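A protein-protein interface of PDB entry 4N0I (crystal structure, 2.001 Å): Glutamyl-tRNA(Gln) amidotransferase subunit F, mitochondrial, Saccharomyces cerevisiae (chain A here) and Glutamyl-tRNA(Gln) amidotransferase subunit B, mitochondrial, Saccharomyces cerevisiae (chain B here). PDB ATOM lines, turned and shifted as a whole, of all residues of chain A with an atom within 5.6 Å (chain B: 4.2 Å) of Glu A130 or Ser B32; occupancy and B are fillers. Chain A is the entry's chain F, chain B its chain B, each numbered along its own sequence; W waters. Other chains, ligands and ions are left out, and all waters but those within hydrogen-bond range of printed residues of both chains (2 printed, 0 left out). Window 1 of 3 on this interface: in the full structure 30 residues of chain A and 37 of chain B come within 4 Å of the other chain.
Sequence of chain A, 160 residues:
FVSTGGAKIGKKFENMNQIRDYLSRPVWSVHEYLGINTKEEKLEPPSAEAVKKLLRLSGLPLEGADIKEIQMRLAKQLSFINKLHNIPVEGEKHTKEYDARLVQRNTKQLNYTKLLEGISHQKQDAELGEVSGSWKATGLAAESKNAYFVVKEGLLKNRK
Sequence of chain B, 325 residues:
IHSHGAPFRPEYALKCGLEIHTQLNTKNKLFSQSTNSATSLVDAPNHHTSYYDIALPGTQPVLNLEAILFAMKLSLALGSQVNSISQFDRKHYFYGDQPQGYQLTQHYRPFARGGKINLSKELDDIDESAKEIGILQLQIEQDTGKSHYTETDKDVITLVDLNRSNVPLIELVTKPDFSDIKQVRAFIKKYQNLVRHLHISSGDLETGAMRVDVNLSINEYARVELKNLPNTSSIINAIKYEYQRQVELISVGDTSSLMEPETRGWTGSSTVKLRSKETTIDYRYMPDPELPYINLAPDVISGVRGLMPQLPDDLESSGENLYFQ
The backbone NH of Gln B33 sits at hydrogen-bond distance from the side-chain carboxylate of Glu A130 (2.8 Å).
NE2 of Gln A124 sits at hydrogen-bond distance from O of Gln B33, 2.7 Å away.
The side-chain carboxylate (OE2) of Glu A130 lies within hydrogen-bond range of the side-chain hydroxyl (OG) of Ser B32, 3.4 Å away.
Of the 10 printed residues of chain A, 5 touch a printed residue of chain B.
Printed residues of chain B that touch a printed residue of chain A: Ser B32, Gln B33, Ser B34 and Ser B50.
Among the printed residues, no Asp or Glu carboxylate lies within 4 Å of a Lys or Arg side-chain nitrogen of the other chain.
Water W1 bridges the side-chain hydroxyl of Ser B32 (2.6 Å) and the side-chain carboxylate of Glu A130 (2.7 Å).
Water W2 lies within hydrogen-bond range of O of Leu A128 (3.0 Å) and N of Tyr B52 (3.0 Å).
ND2 of Asn B166 sits close to N of Ser B32, at 3.3 Å.
The backbone NH (N) of Ser B50 sits at hydrogen-bond distance from the side-chain carboxylate (OD2) of Asp B53 (3.1 Å).
The side-chain hydroxyl (OG) of Ser B50 lies close to the backbone NH (N) of Tyr B52 (3.4 Å).
The side-chain hydroxyl of Ser B32 sits at hydrogen-bond distance from the side-chain hydroxyl of Ser B50, at 2.8 Å.
The side-chain amide nitrogen (NE2) of Gln A124 sits at hydrogen-bond distance from the backbone carbonyl oxygen (O) of Glu A130.
The side-chain hydroxyl (OG) of Ser B34 sits at hydrogen-bond distance from the side-chain carboxylate (OD2) of Asp B53 (2.6 Å).
Printed residues of chain B within 4 Å of Gln A124: Gln B33 and Ser B34.
Of the printed residues of chain B, Gly A129 touches Ser B50.
Of the printed residues of chain B, Glu A130 touches Ser B32 (3.4 Å), Gln B33 (2.8 Å), Ser B34 (3.6 Å) and Ser B50 (3.8 Å).
Val A131 touches none of the printed residues of chain B.
Phe B31 touches none of the printed residues of chain A.
Ser B32 touches one residue of chain A.
Of the printed residues of chain A, Gln B33 touches Lys A123, Gln A124 and Glu A130.
Printed residues of chain A within 4 Å of Ser B50: Leu A128, Gly A129 and Glu A130.
Among the printed residues, pairs that only touch across the chains: Lys A123 with Gln B33 (3.8 Å), Gln A124 with Ser B34 (3.6 Å), Leu A128 with Ser B50 (3.6 Å), Gly A129 with Ser B50 (3.4 Å), Glu A130 with Ser B34 (3.6 Å) and Glu A130 with Ser B50 (3.8 Å).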
ATOM      1  N   LYS A 123       0.352  -9.104  17.487  1.00  0.00           N
ATOM      2  CA  LYS A 123      -0.319  -8.458  16.356  1.00  0.00           C
ATOM      3  C   LYS A 123      -0.367  -6.959  16.591  1.00  0.00           C
ATOM      4  O   LYS A 123      -0.208  -6.506  17.720  1.00  0.00           O
ATOM      5  CB  LYS A 123      -1.738  -8.991  16.203  1.00  0.00           C
ATOM      6  CG  LYS A 123      -2.678  -8.552  17.307  1.00  0.00           C
ATOM      7  CD  LYS A 123      -4.067  -9.142  17.121  1.00  0.00           C
ATOM      8  CE  LYS A 123      -4.068 -10.649  17.357  1.00  0.00           C
ATOM      9  NZ  LYS A 123      -3.827 -11.014  18.788  1.00  0.00           N
ATOM     10  N   GLN A 124      -0.599  -6.178  15.539  1.00  0.00           N
ATOM     11  CA  GLN A 124      -0.613  -4.727  15.695  1.00  0.00           C
ATOM     12  C   GLN A 124      -1.968  -4.226  16.169  1.00  0.00           C
ATOM     13  O   GLN A 124      -2.995  -4.502  15.557  1.00  0.00           O
ATOM     14  CB  GLN A 124      -0.182  -4.036  14.396  1.00  0.00           C
ATOM     15  CG  GLN A 124       1.118  -4.610  13.847  1.00  0.00           C
ATOM     16  CD  GLN A 124       1.710  -3.766  12.749  1.00  0.00           C
ATOM     17  OE1 GLN A 124       1.022  -3.394  11.800  1.00  0.00           O
ATOM     18  NE2 GLN A 124       2.992  -3.448  12.877  1.00  0.00           N
ATOM     19  N   ASP A 125      -1.954  -3.483  17.271  1.00  0.00           N
ATOM     20  CA  ASP A 125      -3.169  -3.017  17.922  1.00  0.00           C
ATOM     21  C   ASP A 125      -3.431  -1.580  17.472  1.00  0.00           C
ATOM     22  O   ASP A 125      -2.589  -0.696  17.653  1.00  0.00           O
ATOM     23  CB  ASP A 125      -2.965  -3.102  19.445  1.00  0.00           C
ATOM     24  CG  ASP A 125      -4.225  -2.781  20.254  1.00  0.00           C
ATOM     25  OD1 ASP A 125      -5.187  -2.187  19.722  1.00  0.00           O
ATOM     26  OD2 ASP A 125      -4.230  -3.119  21.461  1.00  0.00           O
ATOM     27  N   ALA A 126      -4.595  -1.346  16.873  1.00  0.00           N
ATOM     28  CA  ALA A 126      -4.963  -0.006  16.439  1.00  0.00           C
ATOM     29  C   ALA A 126      -5.037   0.934  17.637  1.00  0.00           C
ATOM     30  O   ALA A 126      -4.762   2.122  17.521  1.00  0.00           O
ATOM     31  CB  ALA A 126      -6.288  -0.027  15.701  1.00  0.00           C
ATOM     32  N   LEU A 128      -3.072   1.035  19.932  1.00  0.00           N
ATOM     33  CA  LEU A 128      -1.695   1.442  20.218  1.00  0.00           C
ATOM     34  C   LEU A 128      -1.096   2.256  19.075  1.00  0.00           C
ATOM     35  O   LEU A 128       0.032   2.739  19.175  1.00  0.00           O
ATOM     36  CB  LEU A 128      -0.820   0.219  20.522  1.00  0.00           C
ATOM     37  CG  LEU A 128      -1.159  -0.515  21.816  1.00  0.00           C
ATOM     38  CD1 LEU A 128      -0.364  -1.808  21.962  1.00  0.00           C
ATOM     39  CD2 LEU A 128      -0.904   0.411  22.986  1.00  0.00           C
ATOM     40  N   GLY A 129      -1.855   2.420  17.995  1.00  0.00           N
ATOM     41  CA  GLY A 129      -1.367   3.137  16.824  1.00  0.00           C
ATOM     42  C   GLY A 129      -0.246   2.369  16.139  1.00  0.00           C
ATOM     43  O   GLY A 129       0.619   2.952  15.485  1.00  0.00           O
ATOM     44  N   GLU A 130      -0.253   1.049  16.294  1.00  0.00           N
ATOM     45  CA  GLU A 130       0.851   0.236  15.799  1.00  0.00           C
ATOM     46  C   GLU A 130       0.826  -0.066  14.290  1.00  0.00           C
ATOM     47  O   GLU A 130       1.826  -0.529  13.742  1.00  0.00           O
ATOM     48  CB  GLU A 130       0.946  -1.055  16.594  1.00  0.00           C
ATOM     49  CG  GLU A 130       1.480  -0.842  18.007  1.00  0.00           C
ATOM     50  CD  GLU A 130       1.379  -2.083  18.861  1.00  0.00           C
ATOM     51  OE1 GLU A 130       0.481  -2.914  18.591  1.00  0.00           O
ATOM     52  OE2 GLU A 130       2.192  -2.225  19.808  1.00  0.00           O
ATOM     53  N   VAL A 131      -0.302   0.190  13.622  1.00  0.00           N
ATOM     54  CA  VAL A 131      -0.384  -0.060  12.179  1.00  0.00           C
ATOM     55  C   VAL A 131       0.243   1.119  11.449  1.00  0.00           C
ATOM     56  O   VAL A 131      -0.125   2.258  11.691  1.00  0.00           O
ATOM     57  CB  VAL A 131      -1.844  -0.288  11.704  1.00  0.00           C
ATOM     58  CG1 VAL A 131      -1.897  -0.487  10.191  1.00  0.00           C
ATOM     59  CG2 VAL A 131      -2.451  -1.492  12.423  1.00  0.00           C
ATOM     60  N   SER A 132       1.209   0.845  10.576  1.00  0.00           N
ATOM     61  CA  SER A 132       1.935   1.915   9.889  1.00  0.00           C
ATOM     62  C   SER A 132       1.005   2.888   9.171  1.00  0.00           C
ATOM     63  O   SER A 132       0.086   2.478   8.459  1.00  0.00           O
ATOM     64  CB  SER A 132       2.946   1.334   8.898  1.00  0.00           C
ATOM     65  OG  SER A 132       3.890   0.514   9.565  1.00  0.00           O
ATOM     66  N   SER A 134      -1.233   4.786  10.373  1.00  0.00           N
ATOM     67  CA  SER A 134      -2.598   4.811  10.900  1.00  0.00           C
ATOM     68  C   SER A 134      -2.904   6.126  11.604  1.00  0.00           C
ATOM     69  O   SER A 134      -4.061   6.437  11.881  1.00  0.00           O
ATOM     70  CB  SER A 134      -2.841   3.641  11.859  1.00  0.00           C
ATOM     71  OG  SER A 134      -2.120   3.809  13.071  1.00  0.00           O
ATOM     72  N   LYS B  29       8.892  -4.226  16.264  1.00  0.00           N
ATOM     73  CA  LYS B  29       9.933  -3.608  17.082  1.00  0.00           C
ATOM     74  C   LYS B  29      10.068  -4.249  18.473  1.00  0.00           C
ATOM     75  O   LYS B  29       9.344  -5.182  18.812  1.00  0.00           O
ATOM     76  CB  LYS B  29       9.686  -2.097  17.199  1.00  0.00           C
ATOM     77  CG  LYS B  29       9.857  -1.326  15.862  1.00  0.00           C
ATOM     78  CD  LYS B  29       9.809   0.198  16.100  1.00  0.00           C
ATOM     79  CE  LYS B  29       9.741   1.008  14.790  1.00  0.00           C
ATOM     80  NZ  LYS B  29       9.690   2.500  15.077  1.00  0.00           N
ATOM     81  N   LEU B  30      10.966  -3.707  19.286  1.00  0.00           N
ATOM     82  CA  LEU B  30      11.351  -4.324  20.547  1.00  0.00           C
ATOM     83  C   LEU B  30      10.303  -4.170  21.645  1.00  0.00           C
ATOM     84  O   LEU B  30       9.896  -5.155  22.253  1.00  0.00           O
ATOM     85  CB  LEU B  30      12.705  -3.784  21.024  1.00  0.00           C
ATOM     86  CG  LEU B  30      13.244  -4.398  22.321  1.00  0.00           C
ATOM     87  CD1 LEU B  30      13.234  -5.937  22.239  1.00  0.00           C
ATOM     88  CD2 LEU B  30      14.656  -3.902  22.603  1.00  0.00           C
ATOM     89  N   PHE B  31       9.857  -2.942  21.893  1.00  0.00           N
ATOM     90  CA  PHE B  31       8.879  -2.719  22.960  1.00  0.00           C
ATOM     91  C   PHE B  31       7.545  -2.219  22.454  1.00  0.00           C
ATOM     92  O   PHE B  31       6.706  -1.740  23.227  1.00  0.00           O
ATOM     93  CB  PHE B  31       9.461  -1.774  24.012  1.00  0.00           C
ATOM     94  CG  PHE B  31      10.537  -2.412  24.820  1.00  0.00           C
ATOM     95  CD1 PHE B  31      10.222  -3.447  25.689  1.00  0.00           C
ATOM     96  CD2 PHE B  31      11.859  -2.039  24.679  1.00  0.00           C
ATOM     97  CE1 PHE B  31      11.202  -4.086  26.436  1.00  0.00           C
ATOM     98  CE2 PHE B  31      12.853  -2.671  25.432  1.00  0.00           C
ATOM     99  CZ  PHE B  31      12.521  -3.703  26.300  1.00  0.00           C
ATOM    100  N   SER B  32       7.344  -2.387  21.155  1.00  0.00           N
ATOM    101  CA  SER B  32       6.092  -2.043  20.503  1.00  0.00           C
ATOM    102  C   SER B  32       5.935  -2.954  19.295  1.00  0.00           C
ATOM    103  O   SER B  32       6.933  -3.408  18.723  1.00  0.00           O
ATOM    104  CB  SER B  32       6.122  -0.580  20.051  1.00  0.00           C
ATOM    105  OG  SER B  32       4.956  -0.226  19.327  1.00  0.00           O
ATOM    106  N   GLN B  33       4.698  -3.205  18.881  1.00  0.00           N
ATOM    107  CA  GLN B  33       4.450  -4.080  17.732  1.00  0.00           C
ATOM    108  C   GLN B  33       4.390  -3.328  16.405  1.00  0.00           C
ATOM    109  O   GLN B  33       3.914  -3.856  15.393  1.00  0.00           O
ATOM    110  CB  GLN B  33       3.206  -4.942  17.946  1.00  0.00           C
ATOM    111  CG  GLN B  33       3.420  -6.030  18.986  1.00  0.00           C
ATOM    112  CD  GLN B  33       4.603  -6.911  18.632  1.00  0.00           C
ATOM    113  OE1 GLN B  33       4.601  -7.567  17.590  1.00  0.00           O
ATOM    114  NE2 GLN B  33       5.637  -6.906  19.477  1.00  0.00           N
ATOM    115  N   SER B  34       4.864  -2.087  16.407  1.00  0.00           N
ATOM    116  CA  SER B  34       4.991  -1.359  15.155  1.00  0.00           C
ATOM    117  C   SER B  34       6.003  -2.083  14.288  1.00  0.00           C
ATOM    118  O   SER B  34       6.809  -2.877  14.785  1.00  0.00           O
ATOM    119  CB  SER B  34       5.408   0.093  15.391  1.00  0.00           C
ATOM    120  OG  SER B  34       6.424   0.142  16.376  1.00  0.00           O
ATOM    121  N   SER B  50       4.482   3.815  16.383  1.00  0.00           N
ATOM    122  CA  SER B  50       3.338   3.735  17.279  1.00  0.00           C
ATOM    123  C   SER B  50       3.304   4.926  18.221  1.00  0.00           C
ATOM    124  O   SER B  50       4.230   5.733  18.227  1.00  0.00           O
ATOM    125  CB  SER B  50       3.428   2.462  18.095  1.00  0.00           C
ATOM    126  OG  SER B  50       4.647   2.471  18.809  1.00  0.00           O
ATOM    127  N   TYR B  52       3.795   4.648  21.303  1.00  0.00           N
ATOM    128  CA  TYR B  52       4.953   4.386  22.151  1.00  0.00           C
ATOM    129  C   TYR B  52       6.261   4.836  21.505  1.00  0.00           C
ATOM    130  O   TYR B  52       7.115   5.407  22.182  1.00  0.00           O
ATOM    131  CB  TYR B  52       5.050   2.896  22.529  1.00  0.00           C
ATOM    132  CG  TYR B  52       6.350   2.569  23.222  1.00  0.00           C
ATOM    133  CD1 TYR B  52       7.469   2.194  22.494  1.00  0.00           C
ATOM    134  CD2 TYR B  52       6.466   2.648  24.608  1.00  0.00           C
ATOM    135  CE1 TYR B  52       8.664   1.920  23.120  1.00  0.00           C
ATOM    136  CE2 TYR B  52       7.669   2.367  25.248  1.00  0.00           C
ATOM    137  CZ  TYR B  52       8.757   1.999  24.492  1.00  0.00           C
ATOM    138  OH  TYR B  52       9.962   1.729  25.082  1.00  0.00           O
ATOM    139  N   ASP B  53       6.422   4.590  20.198  1.00  0.00           N
ATOM    140  CA  ASP B  53       7.659   4.971  19.506  1.00  0.00           C
ATOM    141  C   ASP B  53       7.912   6.479  19.573  1.00  0.00           C
ATOM    142  O   ASP B  53       9.061   6.932  19.560  1.00  0.00           O
ATOM    143  CB  ASP B  53       7.633   4.537  18.038  1.00  0.00           C
ATOM    144  CG  ASP B  53       7.625   3.033  17.863  1.00  0.00           C
ATOM    145  OD1 ASP B  53       7.920   2.269  18.820  1.00  0.00           O
ATOM    146  OD2 ASP B  53       7.288   2.610  16.748  1.00  0.00           O
ATOM    147  N   VAL B  62       5.974  -2.900  25.940  1.00  0.00           N
ATOM    148  CA  VAL B  62       5.642  -4.312  26.095  1.00  0.00           C
ATOM    149  C   VAL B  62       6.637  -5.113  25.263  1.00  0.00           C
ATOM    150  O   VAL B  62       6.807  -4.858  24.067  1.00  0.00           O
ATOM    151  CB  VAL B  62       4.208  -4.623  25.652  1.00  0.00           C
ATOM    152  CG1 VAL B  62       3.945  -6.125  25.661  1.00  0.00           C
ATOM    153  CG2 VAL B  62       3.219  -3.904  26.570  1.00  0.00           C
ATOM    154  N   ASN B 166      13.411   2.145  18.611  1.00  0.00           N
ATOM    155  CA  ASN B 166      12.751   0.997  19.244  1.00  0.00           C
ATOM    156  C   ASN B 166      12.889  -0.314  18.416  1.00  0.00           C
ATOM    157  O   ASN B 166      12.311  -1.344  18.758  1.00  0.00           O
ATOM    158  CB  ASN B 166      11.288   1.341  19.591  1.00  0.00           C
ATOM    159  CG  ASN B 166      10.613   0.293  20.435  1.00  0.00           C
ATOM    160  OD1 ASN B 166      11.202  -0.247  21.366  1.00  0.00           O
ATOM    161  ND2 ASN B 166       9.354   0.005  20.120  1.00  0.00           N
HETATM  162  O   HOH W   1       3.029  -0.016  21.084  1.00  0.00           O
HETATM  163  O   HOH W   2       1.867   2.359  21.481  1.00  0.00           O
